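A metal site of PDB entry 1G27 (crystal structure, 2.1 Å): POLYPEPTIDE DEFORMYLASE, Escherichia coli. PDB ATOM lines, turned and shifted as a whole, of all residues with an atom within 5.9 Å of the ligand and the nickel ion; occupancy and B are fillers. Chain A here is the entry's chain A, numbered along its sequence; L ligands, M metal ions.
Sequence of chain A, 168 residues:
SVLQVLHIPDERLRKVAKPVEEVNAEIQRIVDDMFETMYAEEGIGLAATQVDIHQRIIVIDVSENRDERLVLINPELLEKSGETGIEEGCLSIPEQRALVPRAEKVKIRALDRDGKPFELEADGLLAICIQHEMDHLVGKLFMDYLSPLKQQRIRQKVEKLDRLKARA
The side-chain carboxylate (OE1) of Glu 133 lies close to an oxygen (O2) of the ligand, at 2.7 Å.
An oxygen (O1) of the ligand is in hydrogen-bond range of the backbone NH (N) of Ile 44, 2.8 Å away.
The backbone NH of Leu 91 sits close to an oxygen (O3) of the ligand, at 2.8 Å.
O4 of the ligand lies within hydrogen-bond range of N of Gly 89, at 2.9 Å.
A nitrogen (N1) of the ligand is in hydrogen-bond range of the backbone carbonyl oxygen of Gly 89, at 3.3 Å.
The side-chain amide oxygen (OE1) of Gln 50 lies close to an oxygen (O2) of the ligand (2.9 Å).
A ring nitrogen (NE2) of His 136 lies close to the side-chain amide nitrogen (NE2) of Gln 50, at 3.4 Å.
The side-chain sulfur of Cys 90 lies close to the side-chain amide nitrogen of Gln 50.
The backbone NH (N) of Ser 92 sits close to the side-chain sulfur (SG) of Cys 90 (3.6 Å).
A ring nitrogen (ND1) of His 132 is in hydrogen-bond range of the side-chain carboxylate of Glu 88 (2.5 Å).
The side-chain carboxylate (OE2) of Glu 133 lies within hydrogen-bond range of the side-chain sulfur (SG) of Cys 129 (3.6 Å).
NE2 of Gln 50 lies within hydrogen-bond range of OG of Ser 92.
The side-chain amide oxygen of Gln 50 is in hydrogen-bond range of the backbone NH of Ala 47, 3.2 Å away.
Glu 42 touches the ligand (O to C16, 3.8 Å).
Gly 43 touches the ligand.
Gly 45 touches the ligand.
Glu 88 touches the ligand (C to O4, 3.8 Å).
NH1 of Arg 97 touches C14 of the ligand, 3.7 Å away.
Cys 129 touches the ligand.
Hydrophobic or aromatic side chains within 4 Å of the ligand: Ile 44, Leu 91, His 132 and His 136.
Of the 23 residues printed, 14 come within 4 Å of the ligand.
The nearest printed residue that does not touch the ligand is Ile 128 (4.03 Å).
Residues that only touch the nickel ion: Gln 50.
Four residues have an atom within 4 Å of the nickel ion: Gln 50, Cys 90, His 132 and His 136.
The nickel ion is bound by an oxygen (O3) of the ligand, an oxygen (O2) of the ligand, a ring nitrogen (NE2) of His 136, the side-chain sulfur (SG) of Cys 90 and a ring nitrogen (NE2) of His 132.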
ATOM      1  N   GLU A  41      24.236   0.951  28.864  1.00  0.00           N
ATOM      2  CA  GLU A  41      23.926   1.200  27.439  1.00  0.00           C
ATOM      3  C   GLU A  41      24.755   2.303  26.820  1.00  0.00           C
ATOM      4  O   GLU A  41      24.716   2.489  25.606  1.00  0.00           O
ATOM      5  CB  GLU A  41      22.467   1.509  27.303  1.00  0.00           C
ATOM      6  CG  GLU A  41      21.633   0.298  27.419  1.00  0.00           C
ATOM      7  CD  GLU A  41      22.363  -0.903  26.860  1.00  0.00           C
ATOM      8  OE1 GLU A  41      22.356  -1.965  27.509  1.00  0.00           O
ATOM      9  OE2 GLU A  41      22.997  -0.771  25.781  1.00  0.00           O
ATOM     10  N   GLU A  42      25.497   3.032  27.635  1.00  0.00           N
ATOM     11  CA  GLU A  42      26.351   4.121  27.149  1.00  0.00           C
ATOM     12  C   GLU A  42      25.568   5.312  26.568  1.00  0.00           C
ATOM     13  O   GLU A  42      25.974   5.922  25.567  1.00  0.00           O
ATOM     14  CB  GLU A  42      27.364   3.599  26.120  1.00  0.00           C
ATOM     15  CG  GLU A  42      28.499   2.797  26.725  1.00  0.00           C
ATOM     16  CD  GLU A  42      29.452   2.221  25.666  1.00  0.00           C
ATOM     17  OE1 GLU A  42      28.969   1.635  24.668  1.00  0.00           O
ATOM     18  OE2 GLU A  42      30.689   2.351  25.860  1.00  0.00           O
ATOM     19  N   GLY A  43      24.433   5.637  27.201  1.00  0.00           N
ATOM     20  CA  GLY A  43      23.616   6.758  26.767  1.00  0.00           C
ATOM     21  C   GLY A  43      23.880   7.914  27.708  1.00  0.00           C
ATOM     22  O   GLY A  43      24.507   7.738  28.754  1.00  0.00           O
ATOM     23  N   ILE A  44      23.400   9.097  27.356  1.00  0.00           N
ATOM     24  CA  ILE A  44      23.609  10.277  28.207  1.00  0.00           C
ATOM     25  C   ILE A  44      22.303  10.635  28.883  1.00  0.00           C
ATOM     26  O   ILE A  44      22.245  11.559  29.710  1.00  0.00           O
ATOM     27  CB  ILE A  44      24.111  11.466  27.406  1.00  0.00           C
ATOM     28  CG1 ILE A  44      23.161  11.742  26.248  1.00  0.00           C
ATOM     29  CG2 ILE A  44      25.516  11.167  26.867  1.00  0.00           C
ATOM     30  CD1 ILE A  44      23.522  12.966  25.428  1.00  0.00           C
ATOM     31  N   GLY A  45      21.261   9.872  28.568  1.00  0.00           N
ATOM     32  CA  GLY A  45      19.948  10.076  29.168  1.00  0.00           C
ATOM     33  C   GLY A  45      19.054   8.841  29.023  1.00  0.00           C
ATOM     34  O   GLY A  45      19.314   7.970  28.182  1.00  0.00           O
ATOM     35  N   LEU A  46      18.007   8.780  29.837  1.00  0.00           N
ATOM     36  CA  LEU A  46      17.040   7.697  29.774  1.00  0.00           C
ATOM     37  C   LEU A  46      15.714   8.103  30.388  1.00  0.00           C
ATOM     38  O   LEU A  46      15.661   8.629  31.499  1.00  0.00           O
ATOM     39  CB  LEU A  46      17.584   6.437  30.495  1.00  0.00           C
ATOM     40  CG  LEU A  46      16.944   5.053  30.164  1.00  0.00           C
ATOM     41  CD1 LEU A  46      17.312   4.601  28.773  1.00  0.00           C
ATOM     42  CD2 LEU A  46      17.322   3.985  31.180  1.00  0.00           C
ATOM     43  N   ALA A  47      14.638   7.758  29.687  1.00  0.00           N
ATOM     44  CA  ALA A  47      13.266   8.010  30.141  1.00  0.00           C
ATOM     45  C   ALA A  47      12.628   6.666  30.541  1.00  0.00           C
ATOM     46  O   ALA A  47      12.789   5.679  29.859  1.00  0.00           O
ATOM     47  CB  ALA A  47      12.440   8.657  28.989  1.00  0.00           C
ATOM     48  N   GLN A  50      11.230   4.101  28.068  1.00  0.00           N
ATOM     49  CA  GLN A  50      12.121   3.213  27.321  1.00  0.00           C
ATOM     50  C   GLN A  50      12.349   1.819  27.944  1.00  0.00           C
ATOM     51  O   GLN A  50      12.799   0.895  27.278  1.00  0.00           O
ATOM     52  CB  GLN A  50      13.441   3.886  27.078  1.00  0.00           C
ATOM     53  CG  GLN A  50      13.429   4.914  25.999  1.00  0.00           C
ATOM     54  CD  GLN A  50      14.742   5.631  25.954  1.00  0.00           C
ATOM     55  OE1 GLN A  50      15.102   6.314  26.910  1.00  0.00           O
ATOM     56  NE2 GLN A  50      15.515   5.397  24.880  1.00  0.00           N
ATOM     57  N   ILE A  86      21.368  18.852  16.752  1.00  0.00           N
ATOM     58  CA  ILE A  86      22.564  18.053  16.525  1.00  0.00           C
ATOM     59  C   ILE A  86      22.100  16.736  15.926  1.00  0.00           C
ATOM     60  O   ILE A  86      20.898  16.530  15.756  1.00  0.00           O
ATOM     61  CB  ILE A  86      23.356  17.769  17.831  1.00  0.00           C
ATOM     62  CG1 ILE A  86      22.453  17.209  18.911  1.00  0.00           C
ATOM     63  CG2 ILE A  86      23.972  19.007  18.365  1.00  0.00           C
ATOM     64  CD1 ILE A  86      23.242  16.671  20.128  1.00  0.00           C
ATOM     65  N   GLU A  87      23.024  15.849  15.613  1.00  0.00           N
ATOM     66  CA  GLU A  87      22.652  14.514  15.122  1.00  0.00           C
ATOM     67  C   GLU A  87      22.384  13.660  16.353  1.00  0.00           C
ATOM     68  O   GLU A  87      23.302  13.225  17.028  1.00  0.00           O
ATOM     69  CB  GLU A  87      23.764  13.915  14.290  1.00  0.00           C
ATOM     70  CG  GLU A  87      24.223  14.801  13.182  1.00  0.00           C
ATOM     71  CD  GLU A  87      24.245  14.114  11.852  1.00  0.00           C
ATOM     72  OE1 GLU A  87      23.843  12.928  11.783  1.00  0.00           O
ATOM     73  OE2 GLU A  87      24.673  14.751  10.862  1.00  0.00           O
ATOM     74  N   GLU A  88      21.132  13.507  16.693  1.00  0.00           N
ATOM     75  CA  GLU A  88      20.793  12.775  17.874  1.00  0.00           C
ATOM     76  C   GLU A  88      20.665  11.292  17.556  1.00  0.00           C
ATOM     77  O   GLU A  88      20.351  10.891  16.435  1.00  0.00           O
ATOM     78  CB  GLU A  88      19.463  13.255  18.445  1.00  0.00           C
ATOM     79  CG  GLU A  88      19.389  14.699  18.733  1.00  0.00           C
ATOM     80  CD  GLU A  88      18.104  15.059  19.486  1.00  0.00           C
ATOM     81  OE1 GLU A  88      17.731  16.241  19.504  1.00  0.00           O
ATOM     82  OE2 GLU A  88      17.470  14.144  20.048  1.00  0.00           O
ATOM     83  N   GLY A  89      20.834  10.485  18.574  1.00  0.00           N
ATOM     84  CA  GLY A  89      20.678   9.058  18.455  1.00  0.00           C
ATOM     85  C   GLY A  89      19.783   8.653  19.612  1.00  0.00           C
ATOM     86  O   GLY A  89      19.569   9.451  20.548  1.00  0.00           O
ATOM     87  N   CYS A  90      19.256   7.426  19.561  1.00  0.00           N
ATOM     88  CA  CYS A  90      18.359   6.939  20.603  1.00  0.00           C
ATOM     89  C   CYS A  90      18.652   5.482  20.945  1.00  0.00           C
ATOM     90  O   CYS A  90      18.898   4.677  20.057  1.00  0.00           O
ATOM     91  CB  CYS A  90      16.910   7.055  20.122  1.00  0.00           C
ATOM     92  SG  CYS A  90      15.714   6.924  21.459  1.00  0.00           S
ATOM     93  N   LEU A  91      18.602   5.137  22.233  1.00  0.00           N
ATOM     94  CA  LEU A  91      18.815   3.752  22.651  1.00  0.00           C
ATOM     95  C   LEU A  91      17.695   2.813  22.115  1.00  0.00           C
ATOM     96  O   LEU A  91      17.887   1.606  22.002  1.00  0.00           O
ATOM     97  CB  LEU A  91      18.900   3.669  24.155  1.00  0.00           C
ATOM     98  CG  LEU A  91      20.131   4.330  24.753  1.00  0.00           C
ATOM     99  CD1 LEU A  91      20.143   4.134  26.240  1.00  0.00           C
ATOM    100  CD2 LEU A  91      21.392   3.748  24.157  1.00  0.00           C
ATOM    101  N   SER A  92      16.550   3.404  21.762  1.00  0.00           N
ATOM    102  CA  SER A  92      15.407   2.687  21.246  1.00  0.00           C
ATOM    103  C   SER A  92      15.397   2.562  19.736  1.00  0.00           C
ATOM    104  O   SER A  92      14.563   1.863  19.155  1.00  0.00           O
ATOM    105  CB  SER A  92      14.138   3.318  21.752  1.00  0.00           C
ATOM    106  OG  SER A  92      14.124   3.301  23.179  1.00  0.00           O
ATOM    107  N   GLN A  96      20.946   4.562  14.670  1.00  0.00           N
ATOM    108  CA  GLN A  96      20.471   5.582  13.729  1.00  0.00           C
ATOM    109  C   GLN A  96      20.645   6.954  14.372  1.00  0.00           C
ATOM    110  O   GLN A  96      20.366   7.132  15.563  1.00  0.00           O
ATOM    111  CB  GLN A  96      19.001   5.357  13.368  1.00  0.00           C
ATOM    112  CG  GLN A  96      18.706   4.011  12.681  1.00  0.00           C
ATOM    113  CD  GLN A  96      19.658   3.706  11.533  1.00  0.00           C
ATOM    114  OE1 GLN A  96      19.667   4.395  10.505  1.00  0.00           O
ATOM    115  NE2 GLN A  96      20.480   2.686  11.719  1.00  0.00           N
ATOM    116  N   ARG A  97      21.137   7.909  13.602  1.00  0.00           N
ATOM    117  CA  ARG A  97      21.336   9.269  14.113  1.00  0.00           C
ATOM    118  C   ARG A  97      20.802  10.300  13.112  1.00  0.00           C
ATOM    119  O   ARG A  97      20.852  10.084  11.902  1.00  0.00           O
ATOM    120  CB  ARG A  97      22.834   9.518  14.399  1.00  0.00           C
ATOM    121  CG  ARG A  97      23.404   8.748  15.615  1.00  0.00           C
ATOM    122  CD  ARG A  97      24.055   9.702  16.618  1.00  0.00           C
ATOM    123  NE  ARG A  97      25.271   9.119  17.159  1.00  0.00           N
ATOM    124  CZ  ARG A  97      26.283   9.829  17.669  1.00  0.00           C
ATOM    125  NH1 ARG A  97      27.361   9.205  18.134  1.00  0.00           N
ATOM    126  NH2 ARG A  97      26.196  11.160  17.759  1.00  0.00           N
ATOM    127  N   LEU A 125      24.144  20.878  24.974  1.00  0.00           N
ATOM    128  CA  LEU A 125      23.760  19.471  24.994  1.00  0.00           C
ATOM    129  C   LEU A 125      22.716  19.148  26.040  1.00  0.00           C
ATOM    130  O   LEU A 125      21.770  18.433  25.771  1.00  0.00           O
ATOM    131  CB  LEU A 125      24.994  18.620  25.224  1.00  0.00           C
ATOM    132  CG  LEU A 125      24.798  17.109  25.193  1.00  0.00           C
ATOM    133  CD1 LEU A 125      24.237  16.701  23.835  1.00  0.00           C
ATOM    134  CD2 LEU A 125      26.152  16.425  25.475  1.00  0.00           C
ATOM    135  N   ILE A 128      19.004  19.988  24.857  1.00  0.00           N
ATOM    136  CA  ILE A 128      18.542  19.124  23.780  1.00  0.00           C
ATOM    137  C   ILE A 128      18.191  17.757  24.368  1.00  0.00           C
ATOM    138  O   ILE A 128      17.162  17.184  24.055  1.00  0.00           O
ATOM    139  CB  ILE A 128      19.671  18.943  22.742  1.00  0.00           C
ATOM    140  CG1 ILE A 128      19.919  20.234  21.971  1.00  0.00           C
ATOM    141  CG2 ILE A 128      19.378  17.822  21.777  1.00  0.00           C
ATOM    142  CD1 ILE A 128      21.094  20.121  21.044  1.00  0.00           C
ATOM    143  N   CYS A 129      19.045  17.269  25.264  1.00  0.00           N
ATOM    144  CA  CYS A 129      18.840  15.956  25.888  1.00  0.00           C
ATOM    145  C   CYS A 129      17.561  15.970  26.674  1.00  0.00           C
ATOM    146  O   CYS A 129      16.711  15.062  26.551  1.00  0.00           O
ATOM    147  CB  CYS A 129      20.018  15.570  26.784  1.00  0.00           C
ATOM    148  SG  CYS A 129      19.780  14.010  27.747  1.00  0.00           S
ATOM    149  N   HIS A 132      14.785  15.639  24.345  1.00  0.00           N
ATOM    150  CA  HIS A 132      14.744  14.309  23.787  1.00  0.00           C
ATOM    151  C   HIS A 132      14.006  13.379  24.764  1.00  0.00           C
ATOM    152  O   HIS A 132      13.116  12.639  24.365  1.00  0.00           O
ATOM    153  CB  HIS A 132      16.173  13.837  23.604  1.00  0.00           C
ATOM    154  CG  HIS A 132      16.309  12.520  22.931  1.00  0.00           C
ATOM    155  ND1 HIS A 132      16.828  12.386  21.666  1.00  0.00           N
ATOM    156  CD2 HIS A 132      16.079  11.254  23.380  1.00  0.00           C
ATOM    157  CE1 HIS A 132      16.885  11.107  21.343  1.00  0.00           C
ATOM    158  NE2 HIS A 132      16.461  10.396  22.375  1.00  0.00           N
ATOM    159  N   GLU A 133      14.355  13.460  26.055  1.00  0.00           N
ATOM    160  CA  GLU A 133      13.754  12.623  27.099  1.00  0.00           C
ATOM    161  C   GLU A 133      12.280  12.921  27.353  1.00  0.00           C
ATOM    162  O   GLU A 133      11.472  12.013  27.548  1.00  0.00           O
ATOM    163  CB  GLU A 133      14.526  12.740  28.444  1.00  0.00           C
ATOM    164  CG  GLU A 133      16.084  12.447  28.395  1.00  0.00           C
ATOM    165  CD  GLU A 133      16.459  11.291  27.464  1.00  0.00           C
ATOM    166  OE1 GLU A 133      15.598  10.425  27.206  1.00  0.00           O
ATOM    167  OE2 GLU A 133      17.602  11.253  26.989  1.00  0.00           O
ATOM    168  N   HIS A 136       9.990  11.417  25.005  1.00  0.00           N
ATOM    169  CA  HIS A 136       9.787   9.974  25.250  1.00  0.00           C
ATOM    170  C   HIS A 136       8.568   9.775  26.110  1.00  0.00           C
ATOM    171  O   HIS A 136       7.765   8.904  25.845  1.00  0.00           O
ATOM    172  CB  HIS A 136      11.025   9.323  25.986  1.00  0.00           C
ATOM    173  CG  HIS A 136      12.082   8.786  25.076  1.00  0.00           C
ATOM    174  ND1 HIS A 136      11.813   7.899  24.055  1.00  0.00           N
ATOM    175  CD2 HIS A 136      13.414   9.029  25.021  1.00  0.00           C
ATOM    176  CE1 HIS A 136      12.919   7.618  23.399  1.00  0.00           C
ATOM    177  NE2 HIS A 136      13.912   8.294  23.965  1.00  0.00           N
HETATM  178  C1  LIG L   1      19.656   7.899  24.786  1.00  0.00           C
HETATM  179  C2  LIG L   1      20.215   9.026  23.943  1.00  0.00           C
HETATM  180  C3  LIG L   1      21.703   8.900  23.780  1.00  0.00           C
HETATM  181  O1  LIG L   1      22.408   8.711  24.772  1.00  0.00           O
HETATM  182  N1  LIG L   1      22.190   9.149  22.548  1.00  0.00           N
HETATM  183  C4  LIG L   1      23.593   9.223  22.265  1.00  0.00           C
HETATM  184  C5  LIG L   1      19.789  10.450  24.387  1.00  0.00           C
HETATM  185  C6  LIG L   1      20.240  11.524  23.327  1.00  0.00           C
HETATM  186  C7  LIG L   1      20.237  12.933  23.955  1.00  0.00           C
HETATM  187  C8  LIG L   1      20.138  14.029  22.894  1.00  0.00           C
HETATM  188  N2  LIG L   1      18.212   7.824  24.652  1.00  0.00           N
HETATM  189  C9  LIG L   1      17.432   8.460  25.519  1.00  0.00           C
HETATM  190  O2  LIG L   1      16.210   8.518  25.350  1.00  0.00           O
HETATM  191  O3  LIG L   1      17.547   7.340  23.596  1.00  0.00           O
HETATM  192  C10 LIG L   1      23.763  10.503  21.469  1.00  0.00           C
HETATM  193  N3  LIG L   1      24.601  11.520  21.744  1.00  0.00           N
HETATM  194  C11 LIG L   1      24.580  12.666  20.842  1.00  0.00           C
HETATM  195  C12 LIG L   1      25.526  11.481  22.857  1.00  0.00           C
HETATM  196  O4  LIG L   1      22.988  10.606  20.506  1.00  0.00           O
HETATM  197  C13 LIG L   1      24.189   7.985  21.577  1.00  0.00           C
HETATM  198  C14 LIG L   1      25.695   8.227  21.337  1.00  0.00           C
HETATM  199  C15 LIG L   1      23.510   7.708  20.224  1.00  0.00           C
HETATM  200  C16 LIG L   1      24.011   6.767  22.483  1.00  0.00           C
HETATM  201 NI    NI M   1      15.940   8.247  23.228  1.00  0.00          NI
